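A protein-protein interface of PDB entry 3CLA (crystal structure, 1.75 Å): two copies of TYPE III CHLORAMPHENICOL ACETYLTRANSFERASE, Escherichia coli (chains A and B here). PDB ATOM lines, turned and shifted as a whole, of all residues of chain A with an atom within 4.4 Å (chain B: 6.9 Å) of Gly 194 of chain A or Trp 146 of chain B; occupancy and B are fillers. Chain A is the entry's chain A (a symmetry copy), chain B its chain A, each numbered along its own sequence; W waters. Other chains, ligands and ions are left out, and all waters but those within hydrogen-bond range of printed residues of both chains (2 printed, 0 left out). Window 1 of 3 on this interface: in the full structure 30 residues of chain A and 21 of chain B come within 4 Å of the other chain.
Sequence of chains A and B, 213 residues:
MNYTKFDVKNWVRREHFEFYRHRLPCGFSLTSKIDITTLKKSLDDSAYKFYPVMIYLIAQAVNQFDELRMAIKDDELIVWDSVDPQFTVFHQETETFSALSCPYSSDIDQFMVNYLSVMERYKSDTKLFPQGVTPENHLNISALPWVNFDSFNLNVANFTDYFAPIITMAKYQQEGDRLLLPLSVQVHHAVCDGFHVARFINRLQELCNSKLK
O of Val 147 of chain B sits at hydrogen-bond distance from N of Lys 171 of chain B (3.0 Å). The backbone carbonyl oxygen (O) of Leu 144 of chain B sits at hydrogen-bond distance from the backbone NH (N) of Lys 171 of chain B (3.2 Å). The side-chain amide nitrogen (ND2) of Asn 202 of chain A lies within hydrogen-bond range of the backbone carbonyl oxygen (O) of Ala 198 of chain A, 3.1 Å away. ND1 of His 196 of chain A sits at hydrogen-bond distance from N of Asp 193 of chain A (3.0 Å).
No position is printed for both chains. Of the 9 pairs that touch across the chains among the printed residues, none has its exchanged pair printed and touching as well.
O of Trp 146 of chain B sits at hydrogen-bond distance from ND2 of Asn 202 of chain A.
Gly 194 of chain A touches two residues of chain B. Printed residues of chain A within 4 Å of Phe 97 of chain B: Asp 193 (3.4 Å). Trp 146 of chain B touches four residues of chain A. Printed residues of chain A within 4 Å of Val 147 of chain B: Ala 198 (3.6 Å). The nearest printed residue of chain A that does not touch Trp 146 of chain B is His 196 of chain A (6.0 Å). The nearest printed residue of chain B that does not touch Asp 193 of chain A is Leu 144 of chain B (6.1 Å).
CD1 of Phe 28 of chain A touches CE1 of Phe 152 of chain B, at 3.5 Å. Asp 193 of chain A touches Phe 97 of chain B. Gly 194 of chain A touches Leu 144 of chain B (CA to CD2, 3.8 Å). Gly 194 of chain A touches Trp 146 of chain B. CD2 of Phe 195 of chain A touches CZ of Phe 90 of chain B (3.4 Å). N of Phe 195 of chain A touches CZ3 of Trp 146 of chain B, at 3.5 Å. CB of Ala 198 of chain A touches CB of Trp 146 of chain B, 3.7 Å away. Ala 198 of chain A touches Val 147 of chain B (CB to CG1, 3.6 Å).
Along chain B the printed residues that touch a printed residue of chain A span positions 90 to 152. Of the 8 printed residues of chain A, 6 touch a printed residue of chain B. Hydrophobic or aromatic side chains of chain A that line the printed part of chain B: Phe 28, Phe 195 and Ala 198.
Water W1 lies within hydrogen-bond range of the side-chain carboxylate of Asp 193 of chain A (2.6 Å) and the backbone NH of Phe 97 of chain B (3.1 Å). Water W2 lies within hydrogen-bond range of the side-chain amide oxygen (OD1) of Asn 202 of chain A (2.9 Å), the backbone carbonyl oxygen (O) of Trp 146 of chain B (3.0 Å) and the side-chain amino group (NZ) of Lys 171 of chain B (3.2 Å).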
ATOM      1  N   PHE A  28       5.145 -22.086 -11.314  1.00  0.00           N
ATOM      2  CA  PHE A  28       5.925 -21.099 -12.104  1.00  0.00           C
ATOM      3  C   PHE A  28       6.791 -20.359 -11.062  1.00  0.00           C
ATOM      4  O   PHE A  28       6.441 -20.341  -9.882  1.00  0.00           O
ATOM      5  CB  PHE A  28       5.015 -20.176 -12.926  1.00  0.00           C
ATOM      6  CG  PHE A  28       3.978 -19.387 -12.142  1.00  0.00           C
ATOM      7  CD1 PHE A  28       4.331 -18.121 -11.675  1.00  0.00           C
ATOM      8  CD2 PHE A  28       2.689 -19.876 -11.915  1.00  0.00           C
ATOM      9  CE1 PHE A  28       3.437 -17.337 -10.919  1.00  0.00           C
ATOM     10  CE2 PHE A  28       1.753 -19.112 -11.197  1.00  0.00           C
ATOM     11  CZ  PHE A  28       2.130 -17.831 -10.723  1.00  0.00           C
ATOM     12  N   ASP A 193      -2.276 -18.027  -8.894  1.00  0.00           N
ATOM     13  CA  ASP A 193      -2.302 -17.542 -10.272  1.00  0.00           C
ATOM     14  C   ASP A 193      -1.253 -16.374 -10.277  1.00  0.00           C
ATOM     15  O   ASP A 193      -0.755 -16.050  -9.184  1.00  0.00           O
ATOM     16  CB  ASP A 193      -3.686 -17.091 -10.705  1.00  0.00           C
ATOM     17  CG  ASP A 193      -4.772 -18.166 -10.737  1.00  0.00           C
ATOM     18  OD1 ASP A 193      -5.932 -17.778 -10.471  1.00  0.00           O
ATOM     19  OD2 ASP A 193      -4.404 -19.360 -10.966  1.00  0.00           O
ATOM     20  N   GLY A 194      -1.065 -15.819 -11.472  1.00  0.00           N
ATOM     21  CA  GLY A 194      -0.138 -14.656 -11.539  1.00  0.00           C
ATOM     22  C   GLY A 194      -0.631 -13.487 -10.725  1.00  0.00           C
ATOM     23  O   GLY A 194       0.176 -12.804 -10.045  1.00  0.00           O
ATOM     24  N   PHE A 195      -1.950 -13.290 -10.696  1.00  0.00           N
ATOM     25  CA  PHE A 195      -2.526 -12.238  -9.866  1.00  0.00           C
ATOM     26  C   PHE A 195      -2.071 -12.338  -8.381  1.00  0.00           C
ATOM     27  O   PHE A 195      -1.712 -11.333  -7.770  1.00  0.00           O
ATOM     28  CB  PHE A 195      -4.075 -12.335  -9.881  1.00  0.00           C
ATOM     29  CG  PHE A 195      -4.717 -11.325  -8.964  1.00  0.00           C
ATOM     30  CD1 PHE A 195      -5.360 -11.782  -7.812  1.00  0.00           C
ATOM     31  CD2 PHE A 195      -4.683  -9.976  -9.295  1.00  0.00           C
ATOM     32  CE1 PHE A 195      -5.983 -10.886  -6.916  1.00  0.00           C
ATOM     33  CE2 PHE A 195      -5.321  -9.071  -8.402  1.00  0.00           C
ATOM     34  CZ  PHE A 195      -5.920  -9.533  -7.247  1.00  0.00           C
ATOM     35  N   HIS A 196      -2.180 -13.560  -7.860  1.00  0.00           N
ATOM     36  CA  HIS A 196      -1.836 -13.785  -6.431  1.00  0.00           C
ATOM     37  C   HIS A 196      -0.365 -13.514  -6.105  1.00  0.00           C
ATOM     38  O   HIS A 196      -0.089 -12.962  -5.024  1.00  0.00           O
ATOM     39  CB  HIS A 196      -2.256 -15.185  -5.846  1.00  0.00           C
ATOM     40  CG  HIS A 196      -3.703 -15.496  -6.183  1.00  0.00           C
ATOM     41  ND1 HIS A 196      -4.084 -16.161  -7.305  1.00  0.00           N
ATOM     42  CD2 HIS A 196      -4.868 -15.081  -5.596  1.00  0.00           C
ATOM     43  CE1 HIS A 196      -5.421 -16.228  -7.356  1.00  0.00           C
ATOM     44  NE2 HIS A 196      -5.903 -15.574  -6.320  1.00  0.00           N
ATOM     45  N   VAL A 197       0.491 -13.843  -7.055  1.00  0.00           N
ATOM     46  CA  VAL A 197       1.930 -13.589  -6.843  1.00  0.00           C
ATOM     47  C   VAL A 197       2.197 -12.076  -6.921  1.00  0.00           C
ATOM     48  O   VAL A 197       3.031 -11.568  -6.123  1.00  0.00           O
ATOM     49  CB  VAL A 197       2.715 -14.458  -7.831  1.00  0.00           C
ATOM     50  CG1 VAL A 197       4.210 -14.101  -7.772  1.00  0.00           C
ATOM     51  CG2 VAL A 197       2.598 -15.949  -7.508  1.00  0.00           C
ATOM     52  N   ALA A 198       1.557 -11.419  -7.883  1.00  0.00           N
ATOM     53  CA  ALA A 198       1.777  -9.952  -8.059  1.00  0.00           C
ATOM     54  C   ALA A 198       1.293  -9.233  -6.799  1.00  0.00           C
ATOM     55  O   ALA A 198       1.934  -8.292  -6.341  1.00  0.00           O
ATOM     56  CB  ALA A 198       1.002  -9.466  -9.267  1.00  0.00           C
ATOM     57  N   ASN A 202       3.448  -6.873  -4.563  1.00  0.00           N
ATOM     58  CA  ASN A 202       3.025  -5.481  -4.295  1.00  0.00           C
ATOM     59  C   ASN A 202       2.894  -5.196  -2.829  1.00  0.00           C
ATOM     60  O   ASN A 202       3.306  -4.127  -2.328  1.00  0.00           O
ATOM     61  CB  ASN A 202       1.804  -5.164  -5.132  1.00  0.00           C
ATOM     62  CG  ASN A 202       2.184  -5.064  -6.601  1.00  0.00           C
ATOM     63  OD1 ASN A 202       3.279  -4.633  -7.029  1.00  0.00           O
ATOM     64  ND2 ASN A 202       1.230  -5.459  -7.471  1.00  0.00           N
ATOM     65  N   PHE B  90      -8.730 -11.709 -17.230  1.00  0.00           N
ATOM     66  CA  PHE B  90      -8.923 -11.627 -15.780  1.00  0.00           C
ATOM     67  C   PHE B  90     -10.309 -11.104 -15.464  1.00  0.00           C
ATOM     68  O   PHE B  90     -10.759 -10.117 -16.065  1.00  0.00           O
ATOM     69  CB  PHE B  90      -7.874 -10.697 -15.158  1.00  0.00           C
ATOM     70  CG  PHE B  90      -7.808 -10.592 -13.694  1.00  0.00           C
ATOM     71  CD1 PHE B  90      -7.452 -11.689 -12.915  1.00  0.00           C
ATOM     72  CD2 PHE B  90      -8.203  -9.396 -13.057  1.00  0.00           C
ATOM     73  CE1 PHE B  90      -7.399 -11.558 -11.508  1.00  0.00           C
ATOM     74  CE2 PHE B  90      -8.156  -9.301 -11.653  1.00  0.00           C
ATOM     75  CZ  PHE B  90      -7.703 -10.352 -10.873  1.00  0.00           C
ATOM     76  N   PHE B  97      -9.151 -16.137 -13.620  1.00  0.00           N
ATOM     77  CA  PHE B  97      -9.005 -15.866 -15.078  1.00  0.00           C
ATOM     78  C   PHE B  97      -9.696 -16.978 -15.850  1.00  0.00           C
ATOM     79  O   PHE B  97      -9.986 -18.074 -15.355  1.00  0.00           O
ATOM     80  CB  PHE B  97      -7.524 -15.778 -15.430  1.00  0.00           C
ATOM     81  CG  PHE B  97      -6.793 -17.101 -15.382  1.00  0.00           C
ATOM     82  CD1 PHE B  97      -6.648 -17.873 -16.541  1.00  0.00           C
ATOM     83  CD2 PHE B  97      -6.226 -17.558 -14.189  1.00  0.00           C
ATOM     84  CE1 PHE B  97      -5.977 -19.091 -16.521  1.00  0.00           C
ATOM     85  CE2 PHE B  97      -5.545 -18.780 -14.147  1.00  0.00           C
ATOM     86  CZ  PHE B  97      -5.399 -19.536 -15.322  1.00  0.00           C
ATOM     87  N   ALA B 143      -0.874 -12.582 -19.670  1.00  0.00           N
ATOM     88  CA  ALA B 143      -0.366 -11.257 -19.211  1.00  0.00           C
ATOM     89  C   ALA B 143      -0.478 -11.150 -17.702  1.00  0.00           C
ATOM     90  O   ALA B 143      -1.437 -11.706 -17.134  1.00  0.00           O
ATOM     91  CB  ALA B 143      -1.240 -10.192 -19.875  1.00  0.00           C
ATOM     92  N   LEU B 144       0.515 -10.519 -17.053  1.00  0.00           N
ATOM     93  CA  LEU B 144       0.587 -10.256 -15.623  1.00  0.00           C
ATOM     94  C   LEU B 144       0.777  -8.746 -15.564  1.00  0.00           C
ATOM     95  O   LEU B 144       1.880  -8.283 -15.349  1.00  0.00           O
ATOM     96  CB  LEU B 144       1.674 -10.988 -14.819  1.00  0.00           C
ATOM     97  CG  LEU B 144       1.501 -12.463 -14.486  1.00  0.00           C
ATOM     98  CD1 LEU B 144       1.681 -13.321 -15.727  1.00  0.00           C
ATOM     99  CD2 LEU B 144       2.599 -12.928 -13.509  1.00  0.00           C
ATOM    100  N   PRO B 145      -0.317  -8.040 -15.755  1.00  0.00           N
ATOM    101  CA  PRO B 145      -0.185  -6.571 -15.867  1.00  0.00           C
ATOM    102  C   PRO B 145       0.072  -5.888 -14.557  1.00  0.00           C
ATOM    103  O   PRO B 145       0.418  -4.698 -14.600  1.00  0.00           O
ATOM    104  CB  PRO B 145      -1.525  -6.104 -16.459  1.00  0.00           C
ATOM    105  CG  PRO B 145      -2.452  -7.210 -16.178  1.00  0.00           C
ATOM    106  CD  PRO B 145      -1.655  -8.521 -16.096  1.00  0.00           C
ATOM    107  N   TRP B 146      -0.055  -6.595 -13.454  1.00  0.00           N
ATOM    108  CA  TRP B 146       0.073  -6.031 -12.110  1.00  0.00           C
ATOM    109  C   TRP B 146       1.472  -5.933 -11.553  1.00  0.00           C
ATOM    110  O   TRP B 146       1.673  -5.294 -10.501  1.00  0.00           O
ATOM    111  CB  TRP B 146      -0.793  -6.879 -11.127  1.00  0.00           C
ATOM    112  CG  TRP B 146      -2.110  -7.290 -11.645  1.00  0.00           C
ATOM    113  CD1 TRP B 146      -3.279  -6.575 -11.711  1.00  0.00           C
ATOM    114  CD2 TRP B 146      -2.385  -8.569 -12.248  1.00  0.00           C
ATOM    115  NE1 TRP B 146      -4.252  -7.336 -12.338  1.00  0.00           N
ATOM    116  CE2 TRP B 146      -3.749  -8.553 -12.675  1.00  0.00           C
ATOM    117  CE3 TRP B 146      -1.598  -9.698 -12.509  1.00  0.00           C
ATOM    118  CZ2 TRP B 146      -4.361  -9.613 -13.332  1.00  0.00           C
ATOM    119  CZ3 TRP B 146      -2.213 -10.780 -13.128  1.00  0.00           C
ATOM    120  CH2 TRP B 146      -3.557 -10.759 -13.524  1.00  0.00           C
ATOM    121  N   VAL B 147       2.459  -6.575 -12.159  1.00  0.00           N
ATOM    122  CA  VAL B 147       3.825  -6.547 -11.630  1.00  0.00           C
ATOM    123  C   VAL B 147       4.816  -6.655 -12.800  1.00  0.00           C
ATOM    124  O   VAL B 147       4.566  -7.318 -13.802  1.00  0.00           O
ATOM    125  CB  VAL B 147       4.008  -7.673 -10.583  1.00  0.00           C
ATOM    126  CG1 VAL B 147       3.996  -9.063 -11.231  1.00  0.00           C
ATOM    127  CG2 VAL B 147       5.269  -7.494  -9.750  1.00  0.00           C
ATOM    128  N   ASN B 148       5.953  -6.004 -12.584  1.00  0.00           N
ATOM    129  CA  ASN B 148       7.030  -6.105 -13.578  1.00  0.00           C
ATOM    130  C   ASN B 148       7.866  -7.331 -13.136  1.00  0.00           C
ATOM    131  O   ASN B 148       7.975  -7.592 -11.906  1.00  0.00           O
ATOM    132  CB  ASN B 148       7.863  -4.809 -13.502  1.00  0.00           C
ATOM    133  CG  ASN B 148       9.025  -4.772 -14.475  1.00  0.00           C
ATOM    134  OD1 ASN B 148      10.140  -5.088 -13.995  1.00  0.00           O
ATOM    135  ND2 ASN B 148       8.767  -4.504 -15.749  1.00  0.00           N
ATOM    136  N   PHE B 152      10.457 -15.210 -15.975  1.00  0.00           N
ATOM    137  CA  PHE B 152       9.245 -15.970 -15.671  1.00  0.00           C
ATOM    138  C   PHE B 152       9.523 -17.400 -16.223  1.00  0.00           C
ATOM    139  O   PHE B 152      10.002 -17.461 -17.399  1.00  0.00           O
ATOM    140  CB  PHE B 152       8.012 -15.324 -16.450  1.00  0.00           C
ATOM    141  CG  PHE B 152       6.723 -16.064 -16.137  1.00  0.00           C
ATOM    142  CD1 PHE B 152       5.956 -15.744 -14.975  1.00  0.00           C
ATOM    143  CD2 PHE B 152       6.299 -17.103 -16.991  1.00  0.00           C
ATOM    144  CE1 PHE B 152       4.782 -16.439 -14.655  1.00  0.00           C
ATOM    145  CE2 PHE B 152       5.144 -17.835 -16.674  1.00  0.00           C
ATOM    146  CZ  PHE B 152       4.409 -17.511 -15.504  1.00  0.00           C
ATOM    147  N   ALA B 170       4.804  -9.080 -18.846  1.00  0.00           N
ATOM    148  CA  ALA B 170       4.657  -8.458 -17.499  1.00  0.00           C
ATOM    149  C   ALA B 170       4.207  -7.002 -17.636  1.00  0.00           C
ATOM    150  O   ALA B 170       4.042  -6.536 -18.772  1.00  0.00           O
ATOM    151  CB  ALA B 170       6.036  -8.464 -16.830  1.00  0.00           C
ATOM    152  N   LYS B 171       4.066  -6.262 -16.562  1.00  0.00           N
ATOM    153  CA  LYS B 171       3.763  -4.809 -16.641  1.00  0.00           C
ATOM    154  C   LYS B 171       5.027  -4.148 -17.260  1.00  0.00           C
ATOM    155  O   LYS B 171       6.206  -4.478 -16.910  1.00  0.00           O
ATOM    156  CB  LYS B 171       3.612  -4.342 -15.196  1.00  0.00           C
ATOM    157  CG  LYS B 171       3.478  -2.816 -15.018  1.00  0.00           C
ATOM    158  CD  LYS B 171       3.517  -2.583 -13.496  1.00  0.00           C
ATOM    159  CE  LYS B 171       2.960  -1.172 -13.232  1.00  0.00           C
ATOM    160  NZ  LYS B 171       3.119  -1.030 -11.715  1.00  0.00           N
HETATM  161  O   HOH W   1      -8.286 -18.259 -11.540  1.00  0.00           O
HETATM  162  O   HOH W   2       3.802  -3.344  -9.616  1.00  0.00           O
